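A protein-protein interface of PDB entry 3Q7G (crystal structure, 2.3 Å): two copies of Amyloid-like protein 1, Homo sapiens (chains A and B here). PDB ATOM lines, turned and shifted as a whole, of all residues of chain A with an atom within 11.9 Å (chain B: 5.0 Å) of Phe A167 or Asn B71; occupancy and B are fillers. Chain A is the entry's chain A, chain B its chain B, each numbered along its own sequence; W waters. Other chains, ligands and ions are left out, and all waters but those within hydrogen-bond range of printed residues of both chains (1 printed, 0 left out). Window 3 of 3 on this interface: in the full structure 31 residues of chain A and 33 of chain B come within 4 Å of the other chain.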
ATOM      1  N   THR A 147       5.495  23.602   6.994  1.00  0.00           N
ATOM      2  CA  THR A 147       6.039  23.990   8.283  1.00  0.00           C
ATOM      3  C   THR A 147       5.197  23.344   9.370  1.00  0.00           C
ATOM      4  O   THR A 147       5.714  22.706  10.278  1.00  0.00           O
ATOM      5  CB  THR A 147       5.984  25.502   8.463  1.00  0.00           C
ATOM      6  OG1 THR A 147       6.750  26.137   7.431  1.00  0.00           O
ATOM      7  CG2 THR A 147       6.533  25.866   9.827  1.00  0.00           C
ATOM      8  N   LEU A 148       3.889  23.505   9.255  1.00  0.00           N
ATOM      9  CA  LEU A 148       2.975  22.932  10.229  1.00  0.00           C
ATOM     10  C   LEU A 148       3.075  21.415  10.268  1.00  0.00           C
ATOM     11  O   LEU A 148       3.313  20.822  11.329  1.00  0.00           O
ATOM     12  CB  LEU A 148       1.552  23.347   9.885  1.00  0.00           C
ATOM     13  CG  LEU A 148       1.377  24.868   9.897  1.00  0.00           C
ATOM     14  CD1 LEU A 148       0.107  25.245   9.153  1.00  0.00           C
ATOM     15  CD2 LEU A 148       1.325  25.349  11.344  1.00  0.00           C
ATOM     16  N   HIS A 150       5.370  19.390   9.390  1.00  0.00           N
ATOM     17  CA  HIS A 150       6.633  18.916   9.940  1.00  0.00           C
ATOM     18  C   HIS A 150       6.645  19.041  11.459  1.00  0.00           C
ATOM     19  O   HIS A 150       6.846  18.049  12.173  1.00  0.00           O
ATOM     20  CB  HIS A 150       7.794  19.707   9.346  1.00  0.00           C
ATOM     21  CG  HIS A 150       9.112  19.422  10.002  1.00  0.00           C
ATOM     22  ND1 HIS A 150       9.545  18.142  10.283  1.00  0.00           N
ATOM     23  CD2 HIS A 150      10.098  20.251  10.421  1.00  0.00           C
ATOM     24  CE1 HIS A 150      10.740  18.194  10.845  1.00  0.00           C
ATOM     25  NE2 HIS A 150      11.099  19.462  10.939  1.00  0.00           N
ATOM     26  N   TYR A 151       6.431  20.260  11.951  1.00  0.00           N
ATOM     27  CA  TYR A 151       6.380  20.497  13.389  1.00  0.00           C
ATOM     28  C   TYR A 151       5.402  19.493  13.978  1.00  0.00           C
ATOM     29  O   TYR A 151       5.639  18.890  15.024  1.00  0.00           O
ATOM     30  CB  TYR A 151       5.890  21.937  13.630  1.00  0.00           C
ATOM     31  CG  TYR A 151       5.481  22.242  15.052  1.00  0.00           C
ATOM     32  CD1 TYR A 151       6.320  21.934  16.119  1.00  0.00           C
ATOM     33  CD2 TYR A 151       4.284  22.898  15.316  1.00  0.00           C
ATOM     34  CE1 TYR A 151       5.969  22.282  17.418  1.00  0.00           C
ATOM     35  CE2 TYR A 151       3.920  23.256  16.623  1.00  0.00           C
ATOM     36  CZ  TYR A 151       4.773  22.942  17.664  1.00  0.00           C
ATOM     37  OH  TYR A 151       4.463  23.288  18.958  1.00  0.00           O
ATOM     38  N   GLN A 152       4.294  19.320  13.280  1.00  0.00           N
ATOM     39  CA  GLN A 152       3.266  18.399  13.735  1.00  0.00           C
ATOM     40  C   GLN A 152       3.745  16.941  13.856  1.00  0.00           C
ATOM     41  O   GLN A 152       3.390  16.260  14.821  1.00  0.00           O
ATOM     42  CB  GLN A 152       2.070  18.500  12.787  1.00  0.00           C
ATOM     43  CG  GLN A 152       0.990  17.504  13.033  1.00  0.00           C
ATOM     44  CD  GLN A 152       1.148  16.228  12.212  1.00  0.00           C
ATOM     45  OE1 GLN A 152       0.586  15.197  12.550  1.00  0.00           O
ATOM     46  NE2 GLN A 152       1.901  16.317  11.113  1.00  0.00           N
ATOM     47  N   VAL A 154       7.001  15.959  14.235  1.00  0.00           N
ATOM     48  CA  VAL A 154       8.058  15.939  15.247  1.00  0.00           C
ATOM     49  C   VAL A 154       7.442  15.814  16.647  1.00  0.00           C
ATOM     50  O   VAL A 154       7.987  15.149  17.533  1.00  0.00           O
ATOM     51  CB  VAL A 154       8.889  17.260  15.234  1.00  0.00           C
ATOM     52  CG1 VAL A 154       9.946  17.219  16.353  1.00  0.00           C
ATOM     53  CG2 VAL A 154       9.551  17.458  13.884  1.00  0.00           C
ATOM     54  N   PRO A 159       8.987  14.583  21.272  1.00  0.00           N
ATOM     55  CA  PRO A 159       8.407  15.731  21.973  1.00  0.00           C
ATOM     56  C   PRO A 159       9.430  16.732  22.482  1.00  0.00           C
ATOM     57  O   PRO A 159       9.194  17.943  22.445  1.00  0.00           O
ATOM     58  CB  PRO A 159       7.597  15.084  23.101  1.00  0.00           C
ATOM     59  CG  PRO A 159       8.269  13.757  23.299  1.00  0.00           C
ATOM     60  CD  PRO A 159       8.545  13.325  21.896  1.00  0.00           C
ATOM     61  N   GLU A 160      10.573  16.232  22.936  1.00  0.00           N
ATOM     62  CA  GLU A 160      11.622  17.107  23.442  1.00  0.00           C
ATOM     63  C   GLU A 160      12.147  18.026  22.350  1.00  0.00           C
ATOM     64  O   GLU A 160      12.451  19.203  22.596  1.00  0.00           O
ATOM     65  CB  GLU A 160      12.773  16.267  24.027  1.00  0.00           C
ATOM     66  N   LYS A 161      12.237  17.491  21.132  1.00  0.00           N
ATOM     67  CA  LYS A 161      12.726  18.274  19.980  1.00  0.00           C
ATOM     68  C   LYS A 161      11.650  19.218  19.448  1.00  0.00           C
ATOM     69  O   LYS A 161      11.972  20.266  18.893  1.00  0.00           O
ATOM     70  CB  LYS A 161      13.202  17.341  18.866  1.00  0.00           C
ATOM     71  N   ALA A 162      10.380  18.847  19.616  1.00  0.00           N
ATOM     72  CA  ALA A 162       9.264  19.684  19.160  1.00  0.00           C
ATOM     73  C   ALA A 162       9.251  20.968  19.982  1.00  0.00           C
ATOM     74  O   ALA A 162       9.007  22.064  19.463  1.00  0.00           O
ATOM     75  CB  ALA A 162       7.926  18.946  19.339  1.00  0.00           C
ATOM     76  N   GLN A 163       9.522  20.808  21.274  1.00  0.00           N
ATOM     77  CA  GLN A 163       9.567  21.918  22.201  1.00  0.00           C
ATOM     78  C   GLN A 163      10.649  22.920  21.811  1.00  0.00           C
ATOM     79  O   GLN A 163      10.496  24.127  22.019  1.00  0.00           O
ATOM     80  CB  GLN A 163       9.818  21.388  23.611  1.00  0.00           C
ATOM     81  CG  GLN A 163      10.421  22.393  24.570  1.00  0.00           C
ATOM     82  CD  GLN A 163      10.707  21.760  25.920  1.00  0.00           C
ATOM     83  OE1 GLN A 163      11.404  20.763  26.022  1.00  0.00           O
ATOM     84  NE2 GLN A 163      10.160  22.366  26.963  1.00  0.00           N
ATOM     85  N   GLN A 164      11.728  22.420  21.222  1.00  0.00           N
ATOM     86  CA  GLN A 164      12.829  23.279  20.814  1.00  0.00           C
ATOM     87  C   GLN A 164      12.621  23.960  19.467  1.00  0.00           C
ATOM     88  O   GLN A 164      13.366  24.871  19.107  1.00  0.00           O
ATOM     89  CB  GLN A 164      14.117  22.465  20.820  1.00  0.00           C
ATOM     90  CG  GLN A 164      14.451  21.890  22.182  1.00  0.00           C
ATOM     91  CD  GLN A 164      15.621  20.926  22.129  1.00  0.00           C
ATOM     92  OE1 GLN A 164      16.247  20.740  21.090  1.00  0.00           O
ATOM     93  NE2 GLN A 164      15.910  20.316  23.261  1.00  0.00           N
ATOM     94  N   MET A 165      11.600  23.522  18.731  1.00  0.00           N
ATOM     95  CA  MET A 165      11.271  24.096  17.415  1.00  0.00           C
ATOM     96  C   MET A 165      10.212  25.197  17.519  1.00  0.00           C
ATOM     97  O   MET A 165      10.125  26.061  16.642  1.00  0.00           O
ATOM     98  CB  MET A 165      10.643  23.066  16.478  1.00  0.00           C
ATOM     99  CG  MET A 165      11.345  21.772  16.235  1.00  0.00           C
ATOM    100  SD  MET A 165      10.163  20.737  15.298  1.00  0.00           S
ATOM    101  CE  MET A 165      10.053  21.659  13.802  1.00  0.00           C
ATOM    102  N   ARG A 166       9.375  25.121  18.557  1.00  0.00           N
ATOM    103  CA  ARG A 166       8.265  26.059  18.733  1.00  0.00           C
ATOM    104  C   ARG A 166       8.517  27.464  18.253  1.00  0.00           C
ATOM    105  O   ARG A 166       7.831  27.946  17.347  1.00  0.00           O
ATOM    106  CB  ARG A 166       7.816  26.123  20.186  1.00  0.00           C
ATOM    107  CG  ARG A 166       7.070  24.920  20.653  1.00  0.00           C
ATOM    108  CD  ARG A 166       6.761  25.065  22.114  1.00  0.00           C
ATOM    109  NE  ARG A 166       6.577  23.763  22.748  1.00  0.00           N
ATOM    110  CZ  ARG A 166       6.646  23.558  24.059  1.00  0.00           C
ATOM    111  NH1 ARG A 166       6.894  24.568  24.884  1.00  0.00           N
ATOM    112  NH2 ARG A 166       6.476  22.343  24.541  1.00  0.00           N
ATOM    113  N   PHE A 167       9.496  28.122  18.862  1.00  0.00           N
ATOM    114  CA  PHE A 167       9.801  29.491  18.504  1.00  0.00           C
ATOM    115  C   PHE A 167      10.121  29.603  17.021  1.00  0.00           C
ATOM    116  O   PHE A 167       9.544  30.455  16.330  1.00  0.00           O
ATOM    117  CB  PHE A 167      10.977  30.032  19.321  1.00  0.00           C
ATOM    118  CG  PHE A 167      10.884  31.501  19.582  1.00  0.00           C
ATOM    119  CD1 PHE A 167       9.920  31.989  20.461  1.00  0.00           C
ATOM    120  CD2 PHE A 167      11.690  32.402  18.888  1.00  0.00           C
ATOM    121  CE1 PHE A 167       9.749  33.354  20.644  1.00  0.00           C
ATOM    122  CE2 PHE A 167      11.528  33.783  19.063  1.00  0.00           C
ATOM    123  CZ  PHE A 167      10.554  34.256  19.940  1.00  0.00           C
ATOM    124  N   GLN A 168      11.029  28.753  16.541  1.00  0.00           N
ATOM    125  CA  GLN A 168      11.438  28.750  15.141  1.00  0.00           C
ATOM    126  C   GLN A 168      10.231  28.666  14.186  1.00  0.00           C
ATOM    127  O   GLN A 168      10.151  29.405  13.211  1.00  0.00           O
ATOM    128  CB  GLN A 168      12.398  27.589  14.872  1.00  0.00           C
ATOM    129  N   VAL A 169       9.306  27.753  14.473  1.00  0.00           N
ATOM    130  CA  VAL A 169       8.096  27.587  13.669  1.00  0.00           C
ATOM    131  C   VAL A 169       7.267  28.881  13.707  1.00  0.00           C
ATOM    132  O   VAL A 169       6.856  29.407  12.673  1.00  0.00           O
ATOM    133  CB  VAL A 169       7.240  26.428  14.223  1.00  0.00           C
ATOM    134  CG1 VAL A 169       5.937  26.313  13.453  1.00  0.00           C
ATOM    135  CG2 VAL A 169       8.031  25.130  14.163  1.00  0.00           C
ATOM    136  N   HIS A 170       7.036  29.368  14.925  1.00  0.00           N
ATOM    137  CA  HIS A 170       6.280  30.600  15.175  1.00  0.00           C
ATOM    138  C   HIS A 170       6.861  31.752  14.337  1.00  0.00           C
ATOM    139  O   HIS A 170       6.122  32.464  13.641  1.00  0.00           O
ATOM    140  CB  HIS A 170       6.361  30.925  16.677  1.00  0.00           C
ATOM    141  CG  HIS A 170       5.970  32.322  17.040  1.00  0.00           C
ATOM    142  ND1 HIS A 170       4.707  32.827  16.814  1.00  0.00           N
ATOM    143  CD2 HIS A 170       6.646  33.289  17.709  1.00  0.00           C
ATOM    144  CE1 HIS A 170       4.618  34.038  17.334  1.00  0.00           C
ATOM    145  NE2 HIS A 170       5.780  34.342  17.883  1.00  0.00           N
ATOM    146  N   THR A 171       8.184  31.921  14.410  1.00  0.00           N
ATOM    147  CA  THR A 171       8.889  32.959  13.644  1.00  0.00           C
ATOM    148  C   THR A 171       8.704  32.713  12.146  1.00  0.00           C
ATOM    149  O   THR A 171       8.362  33.625  11.383  1.00  0.00           O
ATOM    150  CB  THR A 171      10.420  32.947  13.919  1.00  0.00           C
ATOM    151  OG1 THR A 171      10.681  33.131  15.320  1.00  0.00           O
ATOM    152  CG2 THR A 171      11.116  34.060  13.139  1.00  0.00           C
ATOM    153  N   HIS A 172       8.947  31.473  11.726  1.00  0.00           N
ATOM    154  CA  HIS A 172       8.847  31.082  10.321  1.00  0.00           C
ATOM    155  C   HIS A 172       7.464  31.378   9.742  1.00  0.00           C
ATOM    156  O   HIS A 172       7.359  31.915   8.645  1.00  0.00           O
ATOM    157  CB  HIS A 172       9.192  29.581  10.171  1.00  0.00           C
ATOM    158  CG  HIS A 172       9.346  29.124   8.748  1.00  0.00           C
ATOM    159  ND1 HIS A 172       9.657  27.821   8.416  1.00  0.00           N
ATOM    160  CD2 HIS A 172       9.233  29.792   7.573  1.00  0.00           C
ATOM    161  CE1 HIS A 172       9.726  27.710   7.100  1.00  0.00           C
ATOM    162  NE2 HIS A 172       9.473  28.892   6.565  1.00  0.00           N
ATOM    163  N   LEU A 173       6.406  31.041  10.478  1.00  0.00           N
ATOM    164  CA  LEU A 173       5.052  31.290   9.996  1.00  0.00           C
ATOM    165  C   LEU A 173       4.810  32.801   9.863  1.00  0.00           C
ATOM    166  O   LEU A 173       4.129  33.246   8.944  1.00  0.00           O
ATOM    167  CB  LEU A 173       4.016  30.634  10.930  1.00  0.00           C
ATOM    168  CG  LEU A 173       4.099  29.087  10.945  1.00  0.00           C
ATOM    169  CD1 LEU A 173       3.241  28.464  12.070  1.00  0.00           C
ATOM    170  CD2 LEU A 173       3.649  28.574   9.607  1.00  0.00           C
ATOM    171  N   GLN A 174       5.363  33.598  10.767  1.00  0.00           N
ATOM    172  CA  GLN A 174       5.194  35.047  10.653  1.00  0.00           C
ATOM    173  C   GLN A 174       5.908  35.577   9.396  1.00  0.00           C
ATOM    174  O   GLN A 174       5.382  36.448   8.701  1.00  0.00           O
ATOM    175  CB  GLN A 174       5.745  35.763  11.886  1.00  0.00           C
ATOM    176  CG  GLN A 174       4.795  35.824  13.049  1.00  0.00           C
ATOM    177  CD  GLN A 174       5.327  36.709  14.164  1.00  0.00           C
ATOM    178  OE1 GLN A 174       6.364  36.406  14.772  1.00  0.00           O
ATOM    179  NE2 GLN A 174       4.627  37.817  14.432  1.00  0.00           N
ATOM    180  N   VAL A 175       7.108  35.060   9.122  1.00  0.00           N
ATOM    181  CA  VAL A 175       7.863  35.481   7.935  1.00  0.00           C
ATOM    182  C   VAL A 175       6.961  35.293   6.708  1.00  0.00           C
ATOM    183  O   VAL A 175       6.774  36.207   5.912  1.00  0.00           O
ATOM    184  CB  VAL A 175       9.182  34.639   7.763  1.00  0.00           C
ATOM    185  CG1 VAL A 175       9.794  34.863   6.379  1.00  0.00           C
ATOM    186  CG2 VAL A 175      10.181  35.022   8.843  1.00  0.00           C
ATOM    187  N   ILE A 176       6.379  34.107   6.585  1.00  0.00           N
ATOM    188  CA  ILE A 176       5.502  33.810   5.465  1.00  0.00           C
ATOM    189  C   ILE A 176       4.335  34.792   5.373  1.00  0.00           C
ATOM    190  O   ILE A 176       4.096  35.388   4.316  1.00  0.00           O
ATOM    191  CB  ILE A 176       4.924  32.372   5.551  1.00  0.00           C
ATOM    192  CG1 ILE A 176       6.049  31.339   5.392  1.00  0.00           C
ATOM    193  CG2 ILE A 176       3.853  32.182   4.500  1.00  0.00           C
ATOM    194  CD1 ILE A 176       5.601  29.889   5.603  1.00  0.00           C
ATOM    195  N   TRP B  52      -0.430  33.987  19.003  1.00  0.00           N
ATOM    196  CA  TRP B  52       0.859  34.322  19.570  1.00  0.00           C
ATOM    197  C   TRP B  52       1.481  35.530  18.821  1.00  0.00           C
ATOM    198  O   TRP B  52       2.011  36.464  19.450  1.00  0.00           O
ATOM    199  CB  TRP B  52       1.751  33.086  19.481  1.00  0.00           C
ATOM    200  CG  TRP B  52       3.009  33.158  20.232  1.00  0.00           C
ATOM    201  CD1 TRP B  52       3.453  34.198  20.997  1.00  0.00           C
ATOM    202  CD2 TRP B  52       4.013  32.144  20.318  1.00  0.00           C
ATOM    203  NE1 TRP B  52       4.666  33.896  21.554  1.00  0.00           N
ATOM    204  CE2 TRP B  52       5.035  32.640  21.152  1.00  0.00           C
ATOM    205  CE3 TRP B  52       4.148  30.864  19.772  1.00  0.00           C
ATOM    206  CZ2 TRP B  52       6.179  31.902  21.453  1.00  0.00           C
ATOM    207  CZ3 TRP B  52       5.287  30.127  20.073  1.00  0.00           C
ATOM    208  CH2 TRP B  52       6.287  30.649  20.906  1.00  0.00           C
ATOM    209  N   ASP B  56       2.260  39.180  20.163  1.00  0.00           N
ATOM    210  CA  ASP B  56       3.596  39.742  19.986  1.00  0.00           C
ATOM    211  C   ASP B  56       3.550  41.194  19.510  1.00  0.00           C
ATOM    212  O   ASP B  56       4.239  42.046  20.054  1.00  0.00           O
ATOM    213  CB  ASP B  56       4.392  38.928  18.964  1.00  0.00           C
ATOM    214  CG  ASP B  56       5.116  37.753  19.585  1.00  0.00           C
ATOM    215  OD1 ASP B  56       5.028  37.590  20.826  1.00  0.00           O
ATOM    216  OD2 ASP B  56       5.773  36.992  18.834  1.00  0.00           O
ATOM    217  N   ARG B  67       5.883  40.570  29.215  1.00  0.00           N
ATOM    218  CA  ARG B  67       6.210  40.033  27.913  1.00  0.00           C
ATOM    219  C   ARG B  67       6.539  38.539  28.105  1.00  0.00           C
ATOM    220  O   ARG B  67       6.074  37.678  27.339  1.00  0.00           O
ATOM    221  CB  ARG B  67       7.424  40.764  27.349  1.00  0.00           C
ATOM    222  CG  ARG B  67       7.131  41.544  26.095  1.00  0.00           C
ATOM    223  CD  ARG B  67       7.704  42.941  26.163  1.00  0.00           C
ATOM    224  NE  ARG B  67       9.138  42.978  25.892  1.00  0.00           N
ATOM    225  CZ  ARG B  67      10.053  43.404  26.754  1.00  0.00           C
ATOM    226  NH1 ARG B  67       9.688  43.828  27.953  1.00  0.00           N
ATOM    227  NH2 ARG B  67      11.333  43.424  26.400  1.00  0.00           N
ATOM    228  N   GLN B  68       7.334  38.251  29.141  1.00  0.00           N
ATOM    229  CA  GLN B  68       7.769  36.899  29.457  1.00  0.00           C
ATOM    230  C   GLN B  68       6.572  36.010  29.748  1.00  0.00           C
ATOM    231  O   GLN B  68       6.501  34.893  29.254  1.00  0.00           O
ATOM    232  CB  GLN B  68       8.742  36.910  30.656  1.00  0.00           C
ATOM    233  N   ALA B  69       5.633  36.516  30.542  1.00  0.00           N
ATOM    234  CA  ALA B  69       4.438  35.758  30.875  1.00  0.00           C
ATOM    235  C   ALA B  69       3.652  35.414  29.605  1.00  0.00           C
ATOM    236  O   ALA B  69       3.164  34.298  29.463  1.00  0.00           O
ATOM    237  CB  ALA B  69       3.568  36.539  31.806  1.00  0.00           C
ATOM    238  N   LEU B  70       3.531  36.372  28.691  1.00  0.00           N
ATOM    239  CA  LEU B  70       2.814  36.134  27.433  1.00  0.00           C
ATOM    240  C   LEU B  70       3.444  34.983  26.660  1.00  0.00           C
ATOM    241  O   LEU B  70       2.750  34.110  26.154  1.00  0.00           O
ATOM    242  CB  LEU B  70       2.824  37.386  26.559  1.00  0.00           C
ATOM    243  CG  LEU B  70       1.595  38.277  26.703  1.00  0.00           C
ATOM    244  CD1 LEU B  70       1.812  39.553  25.904  1.00  0.00           C
ATOM    245  CD2 LEU B  70       0.344  37.537  26.213  1.00  0.00           C
ATOM    246  N   ASN B  71       4.766  35.010  26.564  1.00  0.00           N
ATOM    247  CA  ASN B  71       5.480  33.973  25.856  1.00  0.00           C
ATOM    248  C   ASN B  71       5.225  32.600  26.481  1.00  0.00           C
ATOM    249  O   ASN B  71       4.958  31.628  25.771  1.00  0.00           O
ATOM    250  CB  ASN B  71       6.968  34.270  25.853  1.00  0.00           C
ATOM    251  CG  ASN B  71       7.533  34.312  24.456  1.00  0.00           C
ATOM    252  OD1 ASN B  71       8.438  33.541  24.118  1.00  0.00           O
ATOM    253  ND2 ASN B  71       6.993  35.218  23.619  1.00  0.00           N
ATOM    254  N   GLU B  72       5.279  32.535  27.806  1.00  0.00           N
ATOM    255  CA  GLU B  72       5.058  31.284  28.512  1.00  0.00           C
ATOM    256  C   GLU B  72       3.648  30.770  28.242  1.00  0.00           C
ATOM    257  O   GLU B  72       3.430  29.578  28.044  1.00  0.00           O
ATOM    258  CB  GLU B  72       5.281  31.464  30.015  1.00  0.00           C
ATOM    259  N   HIS B  73       2.692  31.683  28.224  1.00  0.00           N
ATOM    260  CA  HIS B  73       1.311  31.318  27.976  1.00  0.00           C
ATOM    261  C   HIS B  73       1.157  30.542  26.666  1.00  0.00           C
ATOM    262  O   HIS B  73       0.533  29.488  26.635  1.00  0.00           O
ATOM    263  CB  HIS B  73       0.465  32.583  27.938  1.00  0.00           C
ATOM    264  CG  HIS B  73      -0.978  32.346  27.626  1.00  0.00           C
ATOM    265  ND1 HIS B  73      -1.508  32.556  26.371  1.00  0.00           N
ATOM    266  CD2 HIS B  73      -2.011  31.967  28.419  1.00  0.00           C
ATOM    267  CE1 HIS B  73      -2.809  32.322  26.412  1.00  0.00           C
ATOM    268  NE2 HIS B  73      -3.139  31.963  27.639  1.00  0.00           N
ATOM    269  N   PHE B  74       1.744  31.058  25.591  1.00  0.00           N
ATOM    270  CA  PHE B  74       1.630  30.381  24.305  1.00  0.00           C
ATOM    271  C   PHE B  74       2.480  29.113  24.202  1.00  0.00           C
ATOM    272  O   PHE B  74       2.033  28.119  23.641  1.00  0.00           O
ATOM    273  CB  PHE B  74       1.928  31.373  23.173  1.00  0.00           C
ATOM    274  CG  PHE B  74       0.804  32.347  22.937  1.00  0.00           C
ATOM    275  CD1 PHE B  74      -0.355  31.941  22.282  1.00  0.00           C
ATOM    276  CD2 PHE B  74       0.858  33.636  23.467  1.00  0.00           C
ATOM    277  CE1 PHE B  74      -1.442  32.788  22.167  1.00  0.00           C
ATOM    278  CE2 PHE B  74      -0.245  34.498  23.352  1.00  0.00           C
ATOM    279  CZ  PHE B  74      -1.395  34.064  22.702  1.00  0.00           C
ATOM    280  N   GLN B  75       3.689  29.146  24.754  1.00  0.00           N
ATOM    281  CA  GLN B  75       4.563  27.978  24.737  1.00  0.00           C
ATOM    282  C   GLN B  75       3.907  26.853  25.538  1.00  0.00           C
ATOM    283  O   GLN B  75       4.092  25.673  25.256  1.00  0.00           O
ATOM    284  CB  GLN B  75       5.916  28.317  25.359  1.00  0.00           C
ATOM    285  CG  GLN B  75       6.780  29.160  24.470  1.00  0.00           C
ATOM    286  CD  GLN B  75       8.044  28.433  24.063  1.00  0.00           C
ATOM    287  OE1 GLN B  75       8.076  27.206  23.984  1.00  0.00           O
ATOM    288  NE2 GLN B  75       9.092  29.196  23.782  1.00  0.00           N
ATOM    289  N   SER B  76       3.120  27.244  26.528  1.00  0.00           N
ATOM    290  CA  SER B  76       2.421  26.309  27.381  1.00  0.00           C
ATOM    291  C   SER B  76       1.211  25.710  26.662  1.00  0.00           C
ATOM    292  O   SER B  76       0.930  24.523  26.779  1.00  0.00           O
ATOM    293  CB  SER B  76       2.000  27.039  28.657  1.00  0.00           C
ATOM    294  OG  SER B  76       1.347  26.171  29.552  1.00  0.00           O
HETATM  295  O   HOH W   1       6.851  37.991  16.918  1.00  0.00           O
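The guanidinium group (NH1) of Arg A166 sits at hydrogen-bond distance from the side-chain amide oxygen (OE1) of Gln B75 (3.0 Å). NE2 of His A170 is in hydrogen-bond range of OD2 of Asp B56, at 2.8 Å.
OG1 of Thr A171 lies within hydrogen-bond range of O of Phe A167 (3.1 Å). The side-chain amide nitrogen (ND2) of Asn B71 lies close to the indole nitrogen (NE1) of Trp B52 (3.4 Å).
Among the printed residues, pairs that only touch across the chains: His A170 with Trp B52 (3.4 Å), Phe A167 with Asn B71 (3.7 Å) and Phe A167 with Trp B52 (3.9 Å).
Gln A168 touches none of the printed residues of chain B. Printed residues of chain B within 4 Å of His A170: Trp B52 and Asp B56. Printed residues of chain A within 4 Å of Trp B52: Phe A167 and His A170. Of the printed residues of chain A, Asp B56 touches His A170. No residue of chain A comes within 4 Å of Ala B69. No residue of chain A comes within 4 Å of Leu B70. Asn B71 touches one residue of chain A. No residue of chain A comes within 4 Å of Glu B72. No residue of chain A comes within 4 Å of Phe B74. Gln B75 touches one residue of chain A. The nearest residue of chain B that does not touch Phe A167 is Gln B75 (4.4 Å). The nearest printed residue of chain B that does not touch Arg A166 is Trp B52 (4.3 Å).
Of the 12 printed residues of chain B, 4 touch a printed residue of chain A. Printed residues of chain B that touch a printed residue of chain A: Trp B52, Asp B56, Asn B71 and Gln B75. Hydrophobic or aromatic side chains of chain A within 4 Å of the printed part of chain B: Phe A167 and His A170. Among the printed residues, no Asp or Glu carboxylate lies within 4 Å of a Lys or Arg side-chain nitrogen of the other chain.
No position is printed for both chains.
Water W1 lies within hydrogen-bond range of the side-chain carboxylate (OD2) of Asp B56 (2.4 Å) and the side-chain amide oxygen (OE1) of Gln A174 (2.7 Å).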
